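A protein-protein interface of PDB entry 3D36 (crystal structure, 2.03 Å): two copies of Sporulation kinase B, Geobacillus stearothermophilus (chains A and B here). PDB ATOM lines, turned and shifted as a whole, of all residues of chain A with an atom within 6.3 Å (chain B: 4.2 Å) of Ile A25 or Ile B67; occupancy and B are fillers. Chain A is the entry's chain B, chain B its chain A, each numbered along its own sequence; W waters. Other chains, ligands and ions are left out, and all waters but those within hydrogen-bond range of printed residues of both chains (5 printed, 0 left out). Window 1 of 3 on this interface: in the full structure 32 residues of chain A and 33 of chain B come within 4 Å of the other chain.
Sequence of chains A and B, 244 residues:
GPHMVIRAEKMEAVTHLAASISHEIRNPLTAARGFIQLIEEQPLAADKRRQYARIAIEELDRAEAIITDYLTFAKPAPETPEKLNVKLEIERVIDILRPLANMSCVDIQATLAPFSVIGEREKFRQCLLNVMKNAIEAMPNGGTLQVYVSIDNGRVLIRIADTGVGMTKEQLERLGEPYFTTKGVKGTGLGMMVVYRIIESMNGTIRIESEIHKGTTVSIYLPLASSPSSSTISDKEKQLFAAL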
ATOM      1  N   SER A  20     -22.519  20.137  -9.646  1.00  0.00           N
ATOM      2  CA  SER A  20     -22.025  21.485  -9.392  1.00  0.00           C
ATOM      3  C   SER A  20     -22.472  22.410 -10.528  1.00  0.00           C
ATOM      4  O   SER A  20     -22.807  21.942 -11.624  1.00  0.00           O
ATOM      5  CB  SER A  20     -20.495  21.490  -9.248  1.00  0.00           C
ATOM      6  OG  SER A  20     -19.858  21.378 -10.512  1.00  0.00           O
ATOM      7  N   ILE A  21     -22.487  23.714 -10.265  1.00  0.00           N
ATOM      8  CA  ILE A  21     -22.955  24.690 -11.259  1.00  0.00           C
ATOM      9  C   ILE A  21     -22.132  24.646 -12.554  1.00  0.00           C
ATOM     10  O   ILE A  21     -22.691  24.696 -13.663  1.00  0.00           O
ATOM     11  CB  ILE A  21     -22.984  26.122 -10.672  1.00  0.00           C
ATOM     12  CG1 ILE A  21     -23.955  26.190  -9.481  1.00  0.00           C
ATOM     13  CG2 ILE A  21     -23.344  27.152 -11.749  1.00  0.00           C
ATOM     14  CD1 ILE A  21     -23.966  27.532  -8.767  1.00  0.00           C
ATOM     15  N   SER A  22     -20.811  24.530 -12.413  1.00  0.00           N
ATOM     16  CA  SER A  22     -19.919  24.500 -13.572  1.00  0.00           C
ATOM     17  C   SER A  22     -20.194  23.264 -14.413  1.00  0.00           C
ATOM     18  O   SER A  22     -20.248  23.351 -15.634  1.00  0.00           O
ATOM     19  CB  SER A  22     -18.442  24.555 -13.159  1.00  0.00           C
ATOM     20  OG  SER A  22     -18.009  23.328 -12.597  1.00  0.00           O
ATOM     21  N   HIS A  23     -20.381  22.124 -13.751  1.00  0.00           N
ATOM     22  CA  HIS A  23     -20.667  20.877 -14.454  1.00  0.00           C
ATOM     23  C   HIS A  23     -21.987  20.967 -15.227  1.00  0.00           C
ATOM     24  O   HIS A  23     -22.061  20.579 -16.399  1.00  0.00           O
ATOM     25  CB  HIS A  23     -20.667  19.691 -13.488  1.00  0.00           C
ATOM     26  CG  HIS A  23     -20.705  18.362 -14.176  1.00  0.00           C
ATOM     27  ND1 HIS A  23     -21.603  17.372 -13.838  1.00  0.00           N
ATOM     28  CD2 HIS A  23     -19.968  17.868 -15.199  1.00  0.00           C
ATOM     29  CE1 HIS A  23     -21.406  16.320 -14.612  1.00  0.00           C
ATOM     30  NE2 HIS A  23     -20.424  16.596 -15.452  1.00  0.00           N
ATOM     31  N   GLU A  24     -23.009  21.507 -14.566  1.00  0.00           N
ATOM     32  CA  GLU A  24     -24.340  21.659 -15.161  1.00  0.00           C
ATOM     33  C   GLU A  24     -24.358  22.597 -16.367  1.00  0.00           C
ATOM     34  O   GLU A  24     -25.092  22.362 -17.331  1.00  0.00           O
ATOM     35  CB  GLU A  24     -25.350  22.130 -14.111  1.00  0.00           C
ATOM     36  CG  GLU A  24     -26.809  21.804 -14.465  1.00  0.00           C
ATOM     37  CD  GLU A  24     -27.135  20.333 -14.326  1.00  0.00           C
ATOM     38  OE1 GLU A  24     -27.545  19.706 -15.338  1.00  0.00           O
ATOM     39  OE2 GLU A  24     -26.981  19.806 -13.207  1.00  0.00           O
ATOM     40  N   ILE A  25     -23.565  23.662 -16.319  1.00  0.00           N
ATOM     41  CA  ILE A  25     -23.499  24.592 -17.448  1.00  0.00           C
ATOM     42  C   ILE A  25     -22.527  24.105 -18.522  1.00  0.00           C
ATOM     43  O   ILE A  25     -22.806  24.248 -19.712  1.00  0.00           O
ATOM     44  CB  ILE A  25     -23.183  26.055 -17.005  1.00  0.00           C
ATOM     45  CG1 ILE A  25     -24.261  26.545 -16.033  1.00  0.00           C
ATOM     46  CG2 ILE A  25     -23.108  27.003 -18.226  1.00  0.00           C
ATOM     47  CD1 ILE A  25     -23.953  27.874 -15.347  1.00  0.00           C
ATOM     48  N   ARG A  26     -21.405  23.521 -18.101  1.00  0.00           N
ATOM     49  CA  ARG A  26     -20.384  23.060 -19.044  1.00  0.00           C
ATOM     50  C   ARG A  26     -20.839  21.931 -19.969  1.00  0.00           C
ATOM     51  O   ARG A  26     -20.408  21.879 -21.114  1.00  0.00           O
ATOM     52  CB  ARG A  26     -19.084  22.673 -18.331  1.00  0.00           C
ATOM     53  CG  ARG A  26     -18.185  23.871 -18.053  1.00  0.00           C
ATOM     54  CD  ARG A  26     -17.009  23.498 -17.188  1.00  0.00           C
ATOM     55  NE  ARG A  26     -16.098  24.634 -17.043  1.00  0.00           N
ATOM     56  CZ  ARG A  26     -15.234  24.791 -16.045  1.00  0.00           C
ATOM     57  NH1 ARG A  26     -15.154  23.888 -15.070  1.00  0.00           N
ATOM     58  NH2 ARG A  26     -14.453  25.863 -16.017  1.00  0.00           N
ATOM     59  N   ASN A  27     -21.681  21.027 -19.473  1.00  0.00           N
ATOM     60  CA  ASN A  27     -22.207  19.951 -20.322  1.00  0.00           C
ATOM     61  C   ASN A  27     -22.838  20.473 -21.633  1.00  0.00           C
ATOM     62  O   ASN A  27     -22.381  20.098 -22.712  1.00  0.00           O
ATOM     63  CB  ASN A  27     -23.160  19.023 -19.552  1.00  0.00           C
ATOM     64  CG  ASN A  27     -22.423  17.966 -18.734  1.00  0.00           C
ATOM     65  OD1 ASN A  27     -21.191  17.868 -18.777  1.00  0.00           O
ATOM     66  ND2 ASN A  27     -23.176  17.167 -17.991  1.00  0.00           N
ATOM     67  N   PRO A  28     -23.880  21.333 -21.546  1.00  0.00           N
ATOM     68  CA  PRO A  28     -24.430  21.872 -22.790  1.00  0.00           C
ATOM     69  C   PRO A  28     -23.481  22.794 -23.562  1.00  0.00           C
ATOM     70  O   PRO A  28     -23.476  22.767 -24.792  1.00  0.00           O
ATOM     71  CB  PRO A  28     -25.682  22.634 -22.334  1.00  0.00           C
ATOM     72  CG  PRO A  28     -25.462  22.931 -20.894  1.00  0.00           C
ATOM     73  CD  PRO A  28     -24.633  21.801 -20.365  1.00  0.00           C
ATOM     74  N   LEU A  29     -22.680  23.588 -22.851  1.00  0.00           N
ATOM     75  CA  LEU A  29     -21.735  24.497 -23.496  1.00  0.00           C
ATOM     76  C   LEU A  29     -20.685  23.761 -24.337  1.00  0.00           C
ATOM     77  O   LEU A  29     -20.379  24.173 -25.466  1.00  0.00           O
ATOM     78  CB  LEU A  29     -21.081  25.422 -22.457  1.00  0.00           C
ATOM     79  CG  LEU A  29     -21.519  26.892 -22.495  1.00  0.00           C
ATOM     80  CD1 LEU A  29     -23.019  27.089 -22.710  1.00  0.00           C
ATOM     81  CD2 LEU A  29     -21.023  27.707 -21.289  1.00  0.00           C
ATOM     82  N   THR A  30     -20.156  22.675 -23.779  1.00  0.00           N
ATOM     83  CA  THR A  30     -19.201  21.799 -24.459  1.00  0.00           C
ATOM     84  C   THR A  30     -19.797  21.219 -25.746  1.00  0.00           C
ATOM     85  O   THR A  30     -19.139  21.195 -26.790  1.00  0.00           O
ATOM     86  CB  THR A  30     -18.766  20.642 -23.517  1.00  0.00           C
ATOM     87  OG1 THR A  30     -18.055  21.190 -22.401  1.00  0.00           O
ATOM     88  CG2 THR A  30     -17.868  19.640 -24.234  1.00  0.00           C
ATOM     89  N   ALA A  63     -28.171  25.718 -21.279  1.00  0.00           N
ATOM     90  CA  ALA A  63     -27.288  26.573 -20.479  1.00  0.00           C
ATOM     91  C   ALA A  63     -28.057  27.760 -19.896  1.00  0.00           C
ATOM     92  O   ALA A  63     -27.891  28.090 -18.726  1.00  0.00           O
ATOM     93  CB  ALA A  63     -26.110  27.061 -21.312  1.00  0.00           C
ATOM     94  N   ILE A  66     -30.317  26.799 -16.955  1.00  0.00           N
ATOM     95  CA  ILE A  66     -29.536  26.591 -15.730  1.00  0.00           C
ATOM     96  C   ILE A  66     -29.125  27.946 -15.129  1.00  0.00           C
ATOM     97  O   ILE A  66     -29.229  28.151 -13.919  1.00  0.00           O
ATOM     98  CB  ILE A  66     -28.261  25.716 -15.979  1.00  0.00           C
ATOM     99  CG1 ILE A  66     -28.618  24.333 -16.562  1.00  0.00           C
ATOM    100  CG2 ILE A  66     -27.415  25.582 -14.685  1.00  0.00           C
ATOM    101  CD1 ILE A  66     -29.659  23.524 -15.759  1.00  0.00           C
ATOM    102  N   ILE A  67     -28.657  28.854 -15.981  1.00  0.00           N
ATOM    103  CA  ILE A  67     -28.342  30.232 -15.568  1.00  0.00           C
ATOM    104  C   ILE A  67     -29.550  30.871 -14.879  1.00  0.00           C
ATOM    105  O   ILE A  67     -29.411  31.500 -13.830  1.00  0.00           O
ATOM    106  CB  ILE A  67     -27.841  31.093 -16.774  1.00  0.00           C
ATOM    107  CG1 ILE A  67     -26.481  30.587 -17.258  1.00  0.00           C
ATOM    108  CG2 ILE A  67     -27.724  32.587 -16.407  1.00  0.00           C
ATOM    109  CD1 ILE A  67     -26.068  31.119 -18.651  1.00  0.00           C
ATOM    110  N   TYR A  70     -30.167  29.258 -11.321  1.00  0.00           N
ATOM    111  CA  TYR A  70     -29.052  29.321 -10.370  1.00  0.00           C
ATOM    112  C   TYR A  70     -28.400  30.699 -10.211  1.00  0.00           C
ATOM    113  O   TYR A  70     -27.880  31.025  -9.134  1.00  0.00           O
ATOM    114  CB  TYR A  70     -27.941  28.353 -10.791  1.00  0.00           C
ATOM    115  CG  TYR A  70     -28.204  26.866 -10.615  1.00  0.00           C
ATOM    116  CD1 TYR A  70     -29.302  26.388  -9.886  1.00  0.00           C
ATOM    117  CD2 TYR A  70     -27.314  25.934 -11.152  1.00  0.00           C
ATOM    118  CE1 TYR A  70     -29.518  25.014  -9.717  1.00  0.00           C
ATOM    119  CE2 TYR A  70     -27.516  24.568 -10.988  1.00  0.00           C
ATOM    120  CZ  TYR A  70     -28.612  24.113 -10.270  1.00  0.00           C
ATOM    121  OH  TYR A  70     -28.790  22.760 -10.104  1.00  0.00           O
ATOM    122  N   LEU A  71     -28.391  31.483 -11.286  1.00  0.00           N
ATOM    123  CA  LEU A  71     -27.501  32.642 -11.362  1.00  0.00           C
ATOM    124  C   LEU A  71     -28.157  33.924 -11.845  1.00  0.00           C
ATOM    125  O   LEU A  71     -27.448  34.845 -12.253  1.00  0.00           O
ATOM    126  CB  LEU A  71     -26.306  32.326 -12.280  1.00  0.00           C
ATOM    127  CG  LEU A  71     -25.402  31.133 -11.965  1.00  0.00           C
ATOM    128  CD1 LEU A  71     -24.494  30.851 -13.152  1.00  0.00           C
ATOM    129  CD2 LEU A  71     -24.603  31.373 -10.685  1.00  0.00           C
ATOM    130  N   ALA B  63     -17.299  32.603 -22.327  1.00  0.00           N
ATOM    131  CA  ALA B  63     -18.205  32.055 -21.318  1.00  0.00           C
ATOM    132  C   ALA B  63     -17.493  31.043 -20.417  1.00  0.00           C
ATOM    133  O   ALA B  63     -17.666  31.072 -19.204  1.00  0.00           O
ATOM    134  CB  ALA B  63     -19.438  31.417 -21.982  1.00  0.00           C
ATOM    135  N   GLU B  64     -16.690  30.167 -21.019  1.00  0.00           N
ATOM    136  CA  GLU B  64     -15.924  29.154 -20.288  1.00  0.00           C
ATOM    137  C   GLU B  64     -14.881  29.784 -19.354  1.00  0.00           C
ATOM    138  O   GLU B  64     -14.662  29.298 -18.239  1.00  0.00           O
ATOM    139  CB  GLU B  64     -15.283  28.155 -21.268  1.00  0.00           C
ATOM    140  CG  GLU B  64     -14.151  27.273 -20.704  1.00  0.00           C
ATOM    141  CD  GLU B  64     -14.612  26.270 -19.639  1.00  0.00           C
ATOM    142  OE1 GLU B  64     -15.832  26.068 -19.465  1.00  0.00           O
ATOM    143  OE2 GLU B  64     -13.738  25.678 -18.968  1.00  0.00           O
ATOM    144  N   ALA B  65     -14.259  30.872 -19.804  1.00  0.00           N
ATOM    145  CA  ALA B  65     -13.297  31.605 -18.979  1.00  0.00           C
ATOM    146  C   ALA B  65     -13.962  32.224 -17.747  1.00  0.00           C
ATOM    147  O   ALA B  65     -13.403  32.173 -16.643  1.00  0.00           O
ATOM    148  CB  ALA B  65     -12.576  32.676 -19.812  1.00  0.00           C
ATOM    149  N   ILE B  66     -15.144  32.808 -17.943  1.00  0.00           N
ATOM    150  CA  ILE B  66     -15.929  33.402 -16.854  1.00  0.00           C
ATOM    151  C   ILE B  66     -16.332  32.329 -15.830  1.00  0.00           C
ATOM    152  O   ILE B  66     -16.196  32.534 -14.622  1.00  0.00           O
ATOM    153  CB  ILE B  66     -17.195  34.158 -17.381  1.00  0.00           C
ATOM    154  CG1 ILE B  66     -16.829  35.280 -18.371  1.00  0.00           C
ATOM    155  CG2 ILE B  66     -18.051  34.699 -16.224  1.00  0.00           C
ATOM    156  CD1 ILE B  66     -15.835  36.314 -17.842  1.00  0.00           C
ATOM    157  N   ILE B  67     -16.810  31.187 -16.325  1.00  0.00           N
ATOM    158  CA  ILE B  67     -17.144  30.038 -15.475  1.00  0.00           C
ATOM    159  C   ILE B  67     -15.940  29.601 -14.626  1.00  0.00           C
ATOM    160  O   ILE B  67     -16.079  29.342 -13.423  1.00  0.00           O
ATOM    161  CB  ILE B  67     -17.718  28.854 -16.317  1.00  0.00           C
ATOM    162  CG1 ILE B  67     -19.048  29.267 -16.954  1.00  0.00           C
ATOM    163  CG2 ILE B  67     -17.876  27.581 -15.470  1.00  0.00           C
ATOM    164  CD1 ILE B  67     -19.598  28.280 -18.008  1.00  0.00           C
ATOM    165  N   THR B  68     -14.766  29.549 -15.250  1.00  0.00           N
ATOM    166  CA  THR B  68     -13.524  29.196 -14.559  1.00  0.00           C
ATOM    167  C   THR B  68     -13.207  30.176 -13.418  1.00  0.00           C
ATOM    168  O   THR B  68     -12.892  29.753 -12.302  1.00  0.00           O
ATOM    169  CB  THR B  68     -12.329  29.119 -15.544  1.00  0.00           C
ATOM    170  OG1 THR B  68     -12.645  28.210 -16.605  1.00  0.00           O
ATOM    171  CG2 THR B  68     -11.054  28.651 -14.841  1.00  0.00           C
ATOM    172  N   ASP B  69     -13.317  31.475 -13.700  1.00  0.00           N
ATOM    173  CA  ASP B  69     -13.016  32.521 -12.710  1.00  0.00           C
ATOM    174  C   ASP B  69     -14.009  32.586 -11.546  1.00  0.00           C
ATOM    175  O   ASP B  69     -13.624  32.914 -10.421  1.00  0.00           O
ATOM    176  CB  ASP B  69     -12.969  33.897 -13.375  1.00  0.00           C
ATOM    177  CG  ASP B  69     -11.727  34.106 -14.218  1.00  0.00           C
ATOM    178  OD1 ASP B  69     -10.612  33.745 -13.786  1.00  0.00           O
ATOM    179  OD2 ASP B  69     -11.870  34.666 -15.315  1.00  0.00           O
ATOM    180  N   TYR B  70     -15.277  32.300 -11.834  1.00  0.00           N
ATOM    181  CA  TYR B  70     -16.375  32.556 -10.902  1.00  0.00           C
ATOM    182  C   TYR B  70     -17.009  31.313 -10.293  1.00  0.00           C
ATOM    183  O   TYR B  70     -17.537  31.366  -9.178  1.00  0.00           O
ATOM    184  CB  TYR B  70     -17.498  33.334 -11.596  1.00  0.00           C
ATOM    185  CG  TYR B  70     -17.239  34.804 -11.861  1.00  0.00           C
ATOM    186  CD1 TYR B  70     -18.133  35.546 -12.638  1.00  0.00           C
ATOM    187  CD2 TYR B  70     -16.118  35.457 -11.342  1.00  0.00           C
ATOM    188  CE1 TYR B  70     -17.922  36.895 -12.889  1.00  0.00           C
ATOM    189  CE2 TYR B  70     -15.895  36.816 -11.599  1.00  0.00           C
ATOM    190  CZ  TYR B  70     -16.809  37.520 -12.369  1.00  0.00           C
ATOM    191  OH  TYR B  70     -16.617  38.851 -12.620  1.00  0.00           O
ATOM    192  N   LEU B  71     -16.994  30.208 -11.036  1.00  0.00           N
ATOM    193  CA  LEU B  71     -17.892  29.095 -10.735  1.00  0.00           C
ATOM    194  C   LEU B  71     -17.261  27.700 -10.779  1.00  0.00           C
ATOM    195  O   LEU B  71     -17.975  26.709 -10.927  1.00  0.00           O
ATOM    196  CB  LEU B  71     -19.096  29.141 -11.691  1.00  0.00           C
ATOM    197  CG  LEU B  71     -19.989  30.389 -11.703  1.00  0.00           C
ATOM    198  CD1 LEU B  71     -20.892  30.376 -12.924  1.00  0.00           C
ATOM    199  CD2 LEU B  71     -20.805  30.506 -10.412  1.00  0.00           C
ATOM    200  N   THR B  72     -15.940  27.616 -10.647  1.00  0.00           N
ATOM    201  CA  THR B  72     -15.246  26.324 -10.717  1.00  0.00           C
ATOM    202  C   THR B  72     -15.725  25.339  -9.640  1.00  0.00           C
ATOM    203  O   THR B  72     -15.842  24.141  -9.899  1.00  0.00           O
ATOM    204  CB  THR B  72     -13.702  26.512 -10.679  1.00  0.00           C
ATOM    205  OG1 THR B  72     -13.280  27.132 -11.901  1.00  0.00           O
ATOM    206  CG2 THR B  72     -12.962  25.178 -10.529  1.00  0.00           C
HETATM  207  O   HOH W   1     -12.661  25.372 -14.056  1.00  0.00           O
HETATM  208  O   HOH W   2     -17.141  21.656  -9.558  1.00  0.00           O
HETATM  209  O   HOH W   3     -13.520  23.147 -18.692  1.00  0.00           O
HETATM  210  O   HOH W   4     -19.173  24.612  -9.960  1.00  0.00           O
HETATM  211  O   HOH W   5     -17.408  23.765 -21.577  1.00  0.00           O
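Water W3 bridges OE2 of Glu B64 (2.6 Å) and NE of Arg A26 (3.4 Å). Water W4 lies within hydrogen-bond range of the backbone carbonyl oxygen of Leu B71 (2.6 Å), the backbone NH of Ser A22 (3.0 Å), the side-chain hydroxyl of Ser A20 (3.4 Å), the backbone carbonyl oxygen of Thr B72 (3.4 Å) and the backbone NH of Ile A21 (3.4 Å). Water W1 bridges the guanidinium group of Arg A26 (2.7 Å) and the side-chain hydroxyl of Thr B72 (2.9 Å). Water W5 bridges OG1 of Thr A30 (2.8 Å) and OE1 of Glu B64 (3.5 Å). Water W2 lies within hydrogen-bond range of the backbone carbonyl oxygen (O) of Thr B72 (2.8 Å) and the side-chain hydroxyl (OG) of Ser A20 (2.9 Å).
Leu B71 touches its own counterpart, Leu A71. Positions printed for both chains: 63, 66, 67, 70 and 71. Of the 9 pairs that touch across the chains among the printed residues, 1 has its exchanged pair printed and touching as well.
The backbone NH (N) of Thr B72 lies within hydrogen-bond range of the backbone carbonyl oxygen (O) of Ile B67. The side-chain hydroxyl of Ser A22 lies within hydrogen-bond range of the side-chain hydroxyl of Ser A20 (3.4 Å). O of Thr B68 is in hydrogen-bond range of OG1 of Thr B72 (2.7 Å). The side-chain hydroxyl (OG1) of Thr B68 sits at hydrogen-bond distance from the backbone carbonyl oxygen (O) of Glu B64 (2.8 Å). OG1 of Thr A30 is in hydrogen-bond range of O of Arg A26 (2.8 Å).
Of chain B, only Ile B67 (3.7 Å) comes within 4 Å of Ile A25. Of the printed residues of chain A, Ile B67 touches Ser A22 (3.8 Å), Ile A25 (3.7 Å), Arg A26 (3.8 Å) and Leu A29 (3.6 Å). Printed residues of chain B within 4 Å of Leu A71: Leu B71 (3.6 Å). Of the printed residues of chain A, Thr B72 touches Ser A22. Of the printed residues of chain A, Thr B68 touches Arg A26. Of the printed residues of chain B, Arg A26 touches Glu B64 (2.8 Å), Ile B67 (3.8 Å) and Thr B68 (3.0 Å). Thr A30 touches none of the printed residues of chain B. The nearest printed residue of chain B that does not touch Ile A25 is Leu B71 (4.6 Å). The nearest residue of chain A that does not touch Ile B67 is Ile A21 (5.9 Å). The nearest printed residue of chain A that does not touch Thr B72 is Arg A26 (4.5 Å).
Of the 16 printed residues of chain A, 5 touch a printed residue of chain B. Printed residues of chain A that touch a printed residue of chain B: Ser A22, Ile A25, Arg A26, Leu A29 and Leu A71. Of the 10 printed residues of chain B, 5 touch a printed residue of chain A. Hydrophobic or aromatic side chains of chain B that line the printed part of chain A: Ile B67 and Leu B71. Among the printed residues, Asp or Glu carboxylates within 4 Å of a Lys or Arg side-chain nitrogen of the other chain: Arg A26 with Glu B64 (2.8 Å).
Ile B67 touches Ser A22. Ser A22 touches Leu B71. O of Thr B72 touches OG of Ser A22, 3.6 Å away. CG2 of Ile A25 touches CD1 of Ile B67, 3.7 Å away. NE of Arg A26 touches CG2 of Ile B67, 3.8 Å away. CD2 of Leu A29 touches CD1 of Ile B67 (3.6 Å). Leu A71 touches Leu B71.
OE1 of Glu B64 is in salt-bridge range of NE of Arg A26, 2.8 Å away. The guanidinium group (NH2) of Arg A26 is in hydrogen-bond range of the side-chain hydroxyl (OG1) of Thr B68 (3.0 Å).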
